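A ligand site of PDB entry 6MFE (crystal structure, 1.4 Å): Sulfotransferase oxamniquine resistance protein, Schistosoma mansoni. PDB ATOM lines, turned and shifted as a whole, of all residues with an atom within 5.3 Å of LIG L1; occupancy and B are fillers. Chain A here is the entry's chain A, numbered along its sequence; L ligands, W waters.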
ATOM      1  N   LEU A  17     -16.255  11.193  11.646  1.00  0.00           N
ATOM      2  CA  LEU A  17     -14.887  11.034  11.161  1.00  0.00           C
ATOM      3  C   LEU A  17     -14.203  12.389  10.917  1.00  0.00           C
ATOM      4  O   LEU A  17     -14.850  13.435  10.819  1.00  0.00           O
ATOM      5  CB  LEU A  17     -14.918  10.238   9.855  1.00  0.00           C
ATOM      6  CG  LEU A  17     -15.361   8.791  10.005  1.00  0.00           C
ATOM      7  CD1 LEU A  17     -15.749   8.144   8.698  1.00  0.00           C
ATOM      8  CD2 LEU A  17     -14.256   7.998  10.696  1.00  0.00           C
ATOM      9  N   PRO A  18     -12.874  12.397  10.858  1.00  0.00           N
ATOM     10  CA  PRO A  18     -12.186  13.632  10.518  1.00  0.00           C
ATOM     11  C   PRO A  18     -12.689  14.211   9.196  1.00  0.00           C
ATOM     12  O   PRO A  18     -13.023  13.474   8.265  1.00  0.00           O
ATOM     13  CB  PRO A  18     -10.717  13.211  10.403  1.00  0.00           C
ATOM     14  CG  PRO A  18     -10.739  11.722  10.339  1.00  0.00           C
ATOM     15  CD  PRO A  18     -11.928  11.291  11.081  1.00  0.00           C
ATOM     16  N   ARG A  19     -12.678  15.549   9.121  1.00  0.00           N
ATOM     17  CA  ARG A  19     -13.132  16.324   7.965  1.00  0.00           C
ATOM     18  C   ARG A  19     -14.644  16.312   7.773  1.00  0.00           C
ATOM     19  O   ARG A  19     -15.127  16.436   6.645  1.00  0.00           O
ATOM     20  CB  ARG A  19     -12.421  15.929   6.678  1.00  0.00           C
ATOM     21  CG  ARG A  19     -10.903  15.852   6.781  1.00  0.00           C
ATOM     22  CD  ARG A  19     -10.237  17.109   7.423  1.00  0.00           C
ATOM     23  NE  ARG A  19     -10.423  18.314   6.623  1.00  0.00           N
ATOM     24  CZ  ARG A  19     -10.107  19.536   7.030  1.00  0.00           C
ATOM     25  NH1 ARG A  19      -9.598  19.744   8.239  1.00  0.00           N
ATOM     26  NH2 ARG A  19     -10.267  20.577   6.222  1.00  0.00           N
ATOM     27  N   THR A  20     -15.397  16.158   8.863  1.00  0.00           N
ATOM     28  CA  THR A  20     -16.858  16.247   8.847  1.00  0.00           C
ATOM     29  C   THR A  20     -17.382  17.352   9.751  1.00  0.00           C
ATOM     30  O   THR A  20     -18.539  17.300  10.173  1.00  0.00           O
ATOM     31  CB  THR A  20     -17.523  14.913   9.240  1.00  0.00           C
ATOM     32  OG1 THR A  20     -17.192  14.579  10.596  1.00  0.00           O
ATOM     33  CG2 THR A  20     -17.083  13.772   8.326  1.00  0.00           C
ATOM     34  N   GLY A  21     -16.557  18.330  10.108  1.00  0.00           N
ATOM     35  CA  GLY A  21     -16.972  19.382  11.025  1.00  0.00           C
ATOM     36  C   GLY A  21     -16.576  19.160  12.467  1.00  0.00           C
ATOM     37  O   GLY A  21     -17.204  19.771  13.354  1.00  0.00           O
ATOM     38  N   THR A  22     -15.563  18.329  12.742  1.00  0.00           N
ATOM     39  CA  THR A  22     -15.218  18.002  14.124  1.00  0.00           C
ATOM     40  C   THR A  22     -14.646  19.208  14.876  1.00  0.00           C
ATOM     41  O   THR A  22     -14.899  19.359  16.072  1.00  0.00           O
ATOM     42  CB  THR A  22     -14.233  16.813  14.196  1.00  0.00           C
ATOM     43  OG1 THR A  22     -12.987  17.178  13.590  1.00  0.00           O
ATOM     44  CG2 THR A  22     -14.805  15.560  13.500  1.00  0.00           C
ATOM     45  N   LYS A  23     -13.837  20.050  14.226  1.00  0.00           N
ATOM     46  CA  LYS A  23     -13.255  21.181  14.934  1.00  0.00           C
ATOM     47  C   LYS A  23     -14.322  22.227  15.249  1.00  0.00           C
ATOM     48  O   LYS A  23     -14.338  22.810  16.350  1.00  0.00           O
ATOM     49  CB  LYS A  23     -12.064  21.743  14.151  1.00  0.00           C
ATOM     50  CG  LYS A  23     -11.299  22.891  14.867  1.00  0.00           C
ATOM     51  CD  LYS A  23     -10.895  22.511  16.274  1.00  0.00           C
ATOM     52  CE  LYS A  23      -9.805  23.383  16.864  1.00  0.00           C
ATOM     53  NZ  LYS A  23     -10.247  24.678  17.427  1.00  0.00           N
ATOM     54  N   SER A  24     -15.231  22.480  14.321  1.00  0.00           N
ATOM     55  CA  SER A  24     -16.330  23.393  14.600  1.00  0.00           C
ATOM     56  C   SER A  24     -17.180  22.873  15.740  1.00  0.00           C
ATOM     57  O   SER A  24     -17.598  23.643  16.604  1.00  0.00           O
ATOM     58  CB  SER A  24     -17.193  23.649  13.372  1.00  0.00           C
ATOM     59  OG  SER A  24     -16.452  24.333  12.380  1.00  0.00           O
ATOM     60  N   HIS A  39     -10.049  16.442  20.755  1.00  0.00           N
ATOM     61  CA  HIS A  39      -9.910  16.582  19.314  1.00  0.00           C
ATOM     62  C   HIS A  39      -8.449  16.297  18.997  1.00  0.00           C
ATOM     63  O   HIS A  39      -7.583  16.408  19.879  1.00  0.00           O
ATOM     64  CB  HIS A  39     -10.279  18.008  18.898  1.00  0.00           C
ATOM     65  CG  HIS A  39     -10.360  18.212  17.420  1.00  0.00           C
ATOM     66  ND1 HIS A  39      -9.291  18.623  16.656  1.00  0.00           N
ATOM     67  CD2 HIS A  39     -11.409  18.110  16.574  1.00  0.00           C
ATOM     68  CE1 HIS A  39      -9.678  18.729  15.394  1.00  0.00           C
ATOM     69  NE2 HIS A  39     -10.955  18.419  15.324  1.00  0.00           N
ATOM     70  N   ARG A 117     -21.320  14.204   5.915  1.00  0.00           N
ATOM     71  CA  ARG A 117     -21.334  15.090   4.756  1.00  0.00           C
ATOM     72  C   ARG A 117     -21.225  14.248   3.502  1.00  0.00           C
ATOM     73  O   ARG A 117     -21.008  13.022   3.547  1.00  0.00           O
ATOM     74  CB  ARG A 117     -20.193  16.118   4.819  1.00  0.00           C
ATOM     75  CG  ARG A 117     -18.826  15.470   4.569  1.00  0.00           C
ATOM     76  CD  ARG A 117     -17.640  16.396   4.753  1.00  0.00           C
ATOM     77  NE  ARG A 117     -17.663  17.541   3.840  1.00  0.00           N
ATOM     78  CZ  ARG A 117     -16.690  18.430   3.745  1.00  0.00           C
ATOM     79  NH1 ARG A 117     -15.590  18.290   4.458  1.00  0.00           N
ATOM     80  NH2 ARG A 117     -16.780  19.454   2.898  1.00  0.00           N
ATOM     81  N   ASP A 121     -16.961  15.212  -1.138  1.00  0.00           N
ATOM     82  CA  ASP A 121     -16.403  16.384  -0.455  1.00  0.00           C
ATOM     83  C   ASP A 121     -15.521  15.932   0.688  1.00  0.00           C
ATOM     84  O   ASP A 121     -14.448  16.518   0.928  1.00  0.00           O
ATOM     85  CB  ASP A 121     -17.515  17.274   0.120  1.00  0.00           C
ATOM     86  CG  ASP A 121     -18.326  18.020  -0.940  1.00  0.00           C
ATOM     87  OD1 ASP A 121     -17.898  18.118  -2.106  1.00  0.00           O
ATOM     88  OD2 ASP A 121     -19.417  18.506  -0.601  1.00  0.00           O
ATOM     89  N   SER A 125     -11.459  16.751   0.959  1.00  0.00           N
ATOM     90  CA  SER A 125     -10.928  17.419   2.138  1.00  0.00           C
ATOM     91  C   SER A 125      -9.857  16.568   2.805  1.00  0.00           C
ATOM     92  O   SER A 125      -8.798  17.079   3.175  1.00  0.00           O
ATOM     93  CB  SER A 125     -12.099  17.673   3.095  1.00  0.00           C
ATOM     94  OG  SER A 125     -11.733  18.460   4.202  1.00  0.00           O
ATOM     95  N   LEU A 205     -23.141  19.105   7.908  1.00  0.00           N
ATOM     96  CA  LEU A 205     -22.517  20.423   7.816  1.00  0.00           C
ATOM     97  C   LEU A 205     -23.569  21.458   7.444  1.00  0.00           C
ATOM     98  O   LEU A 205     -24.356  21.250   6.517  1.00  0.00           O
ATOM     99  CB  LEU A 205     -21.391  20.424   6.778  1.00  0.00           C
ATOM    100  CG  LEU A 205     -20.113  19.691   7.153  1.00  0.00           C
ATOM    101  CD1 LEU A 205     -19.126  19.699   5.966  1.00  0.00           C
ATOM    102  CD2 LEU A 205     -19.494  20.279   8.427  1.00  0.00           C
ATOM    103  N   GLY A 206     -23.622  22.537   8.216  1.00  0.00           N
ATOM    104  CA  GLY A 206     -24.602  23.580   8.005  1.00  0.00           C
ATOM    105  C   GLY A 206     -25.785  23.551   8.942  1.00  0.00           C
ATOM    106  O   GLY A 206     -26.552  24.515   8.965  1.00  0.00           O
ATOM    107  N   TYR A 226     -22.667  29.815  14.916  1.00  0.00           N
ATOM    108  CA  TYR A 226     -22.162  28.462  15.040  1.00  0.00           C
ATOM    109  C   TYR A 226     -20.769  28.466  14.371  1.00  0.00           C
ATOM    110  O   TYR A 226     -20.667  28.990  13.331  1.00  0.00           O
ATOM    111  CB  TYR A 226     -23.064  27.441  14.341  1.00  0.00           C
ATOM    112  CG  TYR A 226     -22.601  25.998  14.545  1.00  0.00           C
ATOM    113  CD1 TYR A 226     -22.938  25.290  15.661  1.00  0.00           C
ATOM    114  CD2 TYR A 226     -21.783  25.391  13.642  1.00  0.00           C
ATOM    115  CE1 TYR A 226     -22.511  24.027  15.842  1.00  0.00           C
ATOM    116  CE2 TYR A 226     -21.341  24.119  13.833  1.00  0.00           C
ATOM    117  CZ  TYR A 226     -21.683  23.461  14.942  1.00  0.00           C
ATOM    118  OH  TYR A 226     -21.236  22.213  15.128  1.00  0.00           O
ATOM    119  N   PRO A 227     -19.770  27.839  14.969  1.00  0.00           N
ATOM    120  CA  PRO A 227     -18.450  27.889  14.328  1.00  0.00           C
ATOM    121  C   PRO A 227     -18.330  27.335  12.902  1.00  0.00           C
ATOM    122  O   PRO A 227     -18.918  26.425  12.578  1.00  0.00           O
ATOM    123  CB  PRO A 227     -17.593  27.035  15.263  1.00  0.00           C
ATOM    124  CG  PRO A 227     -18.300  27.148  16.567  1.00  0.00           C
ATOM    125  CD  PRO A 227     -19.717  27.119  16.241  1.00  0.00           C
ATOM    126  N   CAS A 228     -17.453  27.956  12.111  1.00  0.00           N
ATOM    127  CA  CAS A 228     -17.068  27.506  10.773  1.00  0.00           C
ATOM    128  CB  CAS A 228     -17.718  28.304   9.684  1.00  0.00           C
ATOM    129  C   CAS A 228     -15.565  27.643  10.734  1.00  0.00           C
ATOM    130  O   CAS A 228     -15.052  28.698  10.467  1.00  0.00           O
ATOM    131  SG  CAS A 228     -17.363  27.540   8.124  1.00  0.00           S
ATOM    132 AS   CAS A 228     -15.633  28.661   7.200  1.00  0.00          AS
ATOM    133  CE1 CAS A 228     -13.876  27.856   7.649  1.00  0.00           C
ATOM    134  CE2 CAS A 228     -15.731  27.963   5.328  1.00  0.00           C
ATOM    135  N   VAL A 229     -14.866  26.597  11.055  1.00  0.00           N
ATOM    136  CA  VAL A 229     -13.408  26.636  11.092  1.00  0.00           C
ATOM    137  C   VAL A 229     -12.865  25.347  10.468  1.00  0.00           C
ATOM    138  O   VAL A 229     -13.605  24.469  10.235  1.00  0.00           O
ATOM    139  CB  VAL A 229     -12.854  26.754  12.553  1.00  0.00           C
ATOM    140  CG1 VAL A 229     -13.151  28.095  13.163  1.00  0.00           C
ATOM    141  CG2 VAL A 229     -13.385  25.617  13.385  1.00  0.00           C
ATOM    142  N   ASN A 230     -11.564  25.383  10.158  1.00  0.00           N
ATOM    143  CA  ASN A 230     -10.771  24.244   9.684  1.00  0.00           C
ATOM    144  C   ASN A 230     -11.067  23.818   8.245  1.00  0.00           C
ATOM    145  O   ASN A 230     -10.979  22.698   7.959  1.00  0.00           O
ATOM    146  CB  ASN A 230     -10.868  23.095  10.746  1.00  0.00           C
ATOM    147  CG  ASN A 230      -9.784  22.118  10.728  1.00  0.00           C
ATOM    148  OD1 ASN A 230      -8.774  22.335  10.192  1.00  0.00           O
ATOM    149  ND2 ASN A 230     -10.030  20.987  11.312  1.00  0.00           N
ATOM    150  N   SER A 231     -11.383  24.771   7.386  1.00  0.00           N
ATOM    151  CA  SER A 231     -11.499  24.423   5.975  1.00  0.00           C
ATOM    152  C   SER A 231     -10.144  24.014   5.422  1.00  0.00           C
ATOM    153  O   SER A 231      -9.104  24.426   5.928  1.00  0.00           O
ATOM    154  CB  SER A 231     -11.989  25.607   5.161  1.00  0.00           C
ATOM    155  OG  SER A 231     -11.022  26.638   5.163  1.00  0.00           O
ATOM    156  N   HIS A 232     -10.174  23.196   4.372  1.00  0.00           N
ATOM    157  CA  HIS A 232      -8.904  22.793   3.790  1.00  0.00           C
ATOM    158  C   HIS A 232      -8.114  23.995   3.293  1.00  0.00           C
ATOM    159  O   HIS A 232      -6.885  23.988   3.345  1.00  0.00           O
ATOM    160  CB  HIS A 232      -9.075  21.694   2.732  1.00  0.00           C
ATOM    161  CG  HIS A 232      -9.666  22.133   1.431  1.00  0.00           C
ATOM    162  ND1 HIS A 232      -8.942  22.791   0.460  1.00  0.00           N
ATOM    163  CD2 HIS A 232     -10.906  21.945   0.922  1.00  0.00           C
ATOM    164  CE1 HIS A 232      -9.717  23.018  -0.586  1.00  0.00           C
ATOM    165  NE2 HIS A 232     -10.918  22.508  -0.333  1.00  0.00           N
ATOM    166  N   HIS A 233      -8.784  25.060   2.831  1.00  0.00           N
ATOM    167  CA  HIS A 233      -8.049  26.251   2.403  1.00  0.00           C
ATOM    168  C   HIS A 233      -7.294  26.874   3.573  1.00  0.00           C
ATOM    169  O   HIS A 233      -6.142  27.309   3.422  1.00  0.00           O
ATOM    170  CB  HIS A 233      -9.022  27.272   1.846  1.00  0.00           C
ATOM    171  CG  HIS A 233      -9.667  26.870   0.558  1.00  0.00           C
ATOM    172  ND1 HIS A 233      -8.967  26.714  -0.617  1.00  0.00           N
ATOM    173  CD2 HIS A 233     -10.963  26.607   0.262  1.00  0.00           C
ATOM    174  CE1 HIS A 233      -9.801  26.367  -1.580  1.00  0.00           C
ATOM    175  NE2 HIS A 233     -11.016  26.310  -1.076  1.00  0.00           N
HETATM  176  P1  LIG L   1     -13.511  21.492   3.696  1.00  0.00           P
HETATM  177  O1  LIG L   1     -14.286  20.802   2.615  1.00  0.00           O
HETATM  178  O2  LIG L   1     -12.104  20.968   3.914  1.00  0.00           O
HETATM  179  O3  LIG L   1     -13.483  23.003   3.653  1.00  0.00           O
HETATM  180  P2  LIG L   1     -12.870  18.814  10.561  1.00  0.00           P
HETATM  181  O4  LIG L   1     -13.594  17.564  11.039  1.00  0.00           O
HETATM  182  O5  LIG L   1     -12.880  20.004  11.491  1.00  0.00           O
HETATM  183  O6  LIG L   1     -11.510  18.549  10.012  1.00  0.00           O
HETATM  184  O7  LIG L   1     -13.848  19.278   9.331  1.00  0.00           O
HETATM  185  C1  LIG L   1     -13.480  20.385   8.530  1.00  0.00           C
HETATM  186  C2  LIG L   1     -14.445  20.467   7.331  1.00  0.00           C
HETATM  187  O8  LIG L   1     -15.744  20.873   7.799  1.00  0.00           O
HETATM  188  C3  LIG L   1     -14.021  21.491   6.315  1.00  0.00           C
HETATM  189  O9  LIG L   1     -14.393  21.087   4.986  1.00  0.00           O
HETATM  190  C4  LIG L   1     -14.803  22.712   6.748  1.00  0.00           C
HETATM  191  O10 LIG L   1     -14.928  23.731   5.731  1.00  0.00           O
HETATM  192  C5  LIG L   1     -16.124  22.068   7.113  1.00  0.00           C
HETATM  193  N1  LIG L   1     -16.937  22.894   8.007  1.00  0.00           N
HETATM  194  C6  LIG L   1     -16.649  23.124   9.301  1.00  0.00           C
HETATM  195  N2  LIG L   1     -17.595  23.905   9.874  1.00  0.00           N
HETATM  196  C7  LIG L   1     -18.509  24.161   8.916  1.00  0.00           C
HETATM  197  C8  LIG L   1     -19.744  24.921   8.839  1.00  0.00           C
HETATM  198  N3  LIG L   1     -20.146  25.539   9.960  1.00  0.00           N
HETATM  199  N4  LIG L   1     -20.418  24.954   7.670  1.00  0.00           N
HETATM  200  C9  LIG L   1     -19.970  24.323   6.571  1.00  0.00           C
HETATM  201  N5  LIG L   1     -18.812  23.627   6.559  1.00  0.00           N
HETATM  202  C10 LIG L   1     -18.074  23.491   7.682  1.00  0.00           C
HETATM  203  N1  LG2 L   2      -6.193  13.076  11.894  1.00  0.00           N
HETATM  204  C1  LG2 L   2      -7.881  15.328  12.433  1.00  0.00           C
HETATM  205  O1  LG2 L   2      -8.474  16.537  12.860  1.00  0.00           O
HETATM  206  C2  LG2 L   2      -6.528  15.567  11.775  1.00  0.00           C
HETATM  207  C3  LG2 L   2      -0.935  15.874   8.574  1.00  0.00           C
HETATM  208  C4  LG2 L   2      -1.124  19.476   8.434  1.00  0.00           C
HETATM  209  C5  LG2 L   2      -1.538  20.255   9.639  1.00  0.00           C
HETATM  210  C6  LG2 L   2      -2.872  20.170   9.952  1.00  0.00           C
HETATM  211  C7  LG2 L   2      -3.312  20.827  11.063  1.00  0.00           C
HETATM  212  C8  LG2 L   2      -2.439  21.603  11.824  1.00  0.00           C
HETATM  213  C9  LG2 L   2      -2.688  22.593  14.144  1.00  0.00           C
HETATM  214  C10 LG2 L   2      -1.093  21.727  11.488  1.00  0.00           C
HETATM  215  C11 LG2 L   2      -0.640  21.030  10.381  1.00  0.00           C
HETATM  216  C12 LG2 L   2      -5.731  14.352  11.523  1.00  0.00           C
HETATM  217  C13 LG2 L   2      -4.492  14.458  10.969  1.00  0.00           C
HETATM  218  C14 LG2 L   2      -5.977  16.799  11.415  1.00  0.00           C
HETATM  219  C15 LG2 L   2      -4.698  16.848  10.831  1.00  0.00           C
HETATM  220  C16 LG2 L   2      -3.955  15.672  10.633  1.00  0.00           C
HETATM  221  C17 LG2 L   2      -1.449  16.151   9.985  1.00  0.00           C
HETATM  222  C18 LG2 L   2      -1.336  17.658  10.151  1.00  0.00           C
HETATM  223  C19 LG2 L   2      -1.085  17.215   7.904  1.00  0.00           C
HETATM  224  F1  LG2 L   2      -1.399  22.801  14.205  1.00  0.00           F
HETATM  225  F2  LG2 L   2      -3.354  23.684  14.452  1.00  0.00           F
HETATM  226  F3  LG2 L   2      -3.097  21.701  15.002  1.00  0.00           F
HETATM  227  N2  LG2 L   2      -2.762  15.516  10.009  1.00  0.00           N
HETATM  228  N3  LG2 L   2      -0.693  18.159   8.919  1.00  0.00           N
HETATM  229  O2  LG2 L   2      -7.354  12.625  11.647  1.00  0.00           O
HETATM  230  O3  LG2 L   2      -5.375  12.383  12.517  1.00  0.00           O
HETATM  231  O4  LG2 L   2      -3.113  22.211  12.855  1.00  0.00           O
HETATM  232  O   HOH W   1     -16.671  25.381   3.335  1.00  0.00           O
HETATM  233  O   HOH W   2     -14.069  19.300   0.294  1.00  0.00           O
HETATM  234  O   HOH W   3     -16.165  23.021   2.037  1.00  0.00           O
HETATM  235  O   HOH W   4     -13.575  24.836   1.759  1.00  0.00           O
HETATM  236  O   HOH W   5     -14.588  21.976  11.511  1.00  0.00           O
HETATM  237  O   HOH W   6     -22.469  26.436   6.875  1.00  0.00           O
HETATM  238  O   HOH W   7     -18.566  23.159   3.723  1.00  0.00           O
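C of Pro 18 touches O4 of LIG L1, at 3.9 Å.
Leu 205 touches LIG L1.
SG of CAS 228 touches C8 of LIG L1, 3.6 Å away.
O of Val 229 touches C6 of LIG L1 (3.5 Å).
Ser 231 touches LIG L1.
Hydrophobic or aromatic side chains within 4 Å of LIG L1: Leu 205 and His 232.
Within 4 Å of LIG L1: Pro 18, Arg 19, Thr 20, Gly 21, Thr 22, Lys 23, Ser 24, Arg 117, Ser 125, Leu 205, Pro 227, CAS 228, Val 229, Asn 230, Ser 231 and His 232.
An oxygen (O4) of LIG L1 sits at hydrogen-bond distance from the backbone NH (N) of Arg 19.
OG1 of Thr 22 sits at hydrogen-bond distance from O4 of LIG L1 (2.7 Å).
The backbone NH (N) of Gly 21 is in hydrogen-bond range of an oxygen (O7) of LIG L1, at 3.0 Å.
An oxygen (O5) of LIG L1 is in hydrogen-bond range of the backbone NH (N) of Lys 23, at 2.9 Å.
N of Thr 20 lies within hydrogen-bond range of O4 of LIG L1 (3.2 Å).
N of His 232 lies within hydrogen-bond range of O2 of LIG L1 (3.0 Å).
The side-chain amide nitrogen (ND2) of Asn 230 lies within hydrogen-bond range of an oxygen (O5) of LIG L1 (3.0 Å).
NH1 of Arg 19 lies within salt-bridge range of O6 of LIG L1, at 2.9 Å.
The side-chain hydroxyl (OG) of Ser 24 is in hydrogen-bond range of a nitrogen (N2) of LIG L1 (2.8 Å).
OG of Ser 125 lies within hydrogen-bond range of O2 of LIG L1, 2.6 Å away.
N of Thr 22 sits at hydrogen-bond distance from O4 of LIG L1 (2.7 Å).
The backbone carbonyl oxygen of Pro 227 is in hydrogen-bond range of a nitrogen (N3) of LIG L1.
The guanidinium group of Arg 117 lies within salt-bridge range of an oxygen (O1) of LIG L1.
Water W5 lies within hydrogen-bond range of O5 of LIG L1, N of Ser 24, O of Val 229 and N of Lys 23.
Water W2 bridges O1 of LIG L1 and O of Asp 121.
The guanidinium group (NH1) of Arg 117 lies within hydrogen-bond range of the backbone carbonyl oxygen (O) of Arg 19, at 2.9 Å.
OG of Ser 24 is in hydrogen-bond range of O of Pro 227 (3.2 Å).
The guanidinium group of Arg 19 is in hydrogen-bond range of the backbone carbonyl oxygen of Asn 230 (2.8 Å).
OG1 of Thr 22 sits at hydrogen-bond distance from NE2 of His 39 (2.9 Å).
N of Lys 23 sits at hydrogen-bond distance from NE2 of His 39 (3.5 Å).
The backbone carbonyl oxygen (O) of Leu 17 is in hydrogen-bond range of the side-chain hydroxyl (OG1) of Thr 20 (2.6 Å).
The side-chain hydroxyl (OG) of Ser 125 is in hydrogen-bond range of the guanidinium group (NE) of Arg 19 (2.8 Å).
The backbone NH of Val 229 is in hydrogen-bond range of the side-chain hydroxyl of Ser 24.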
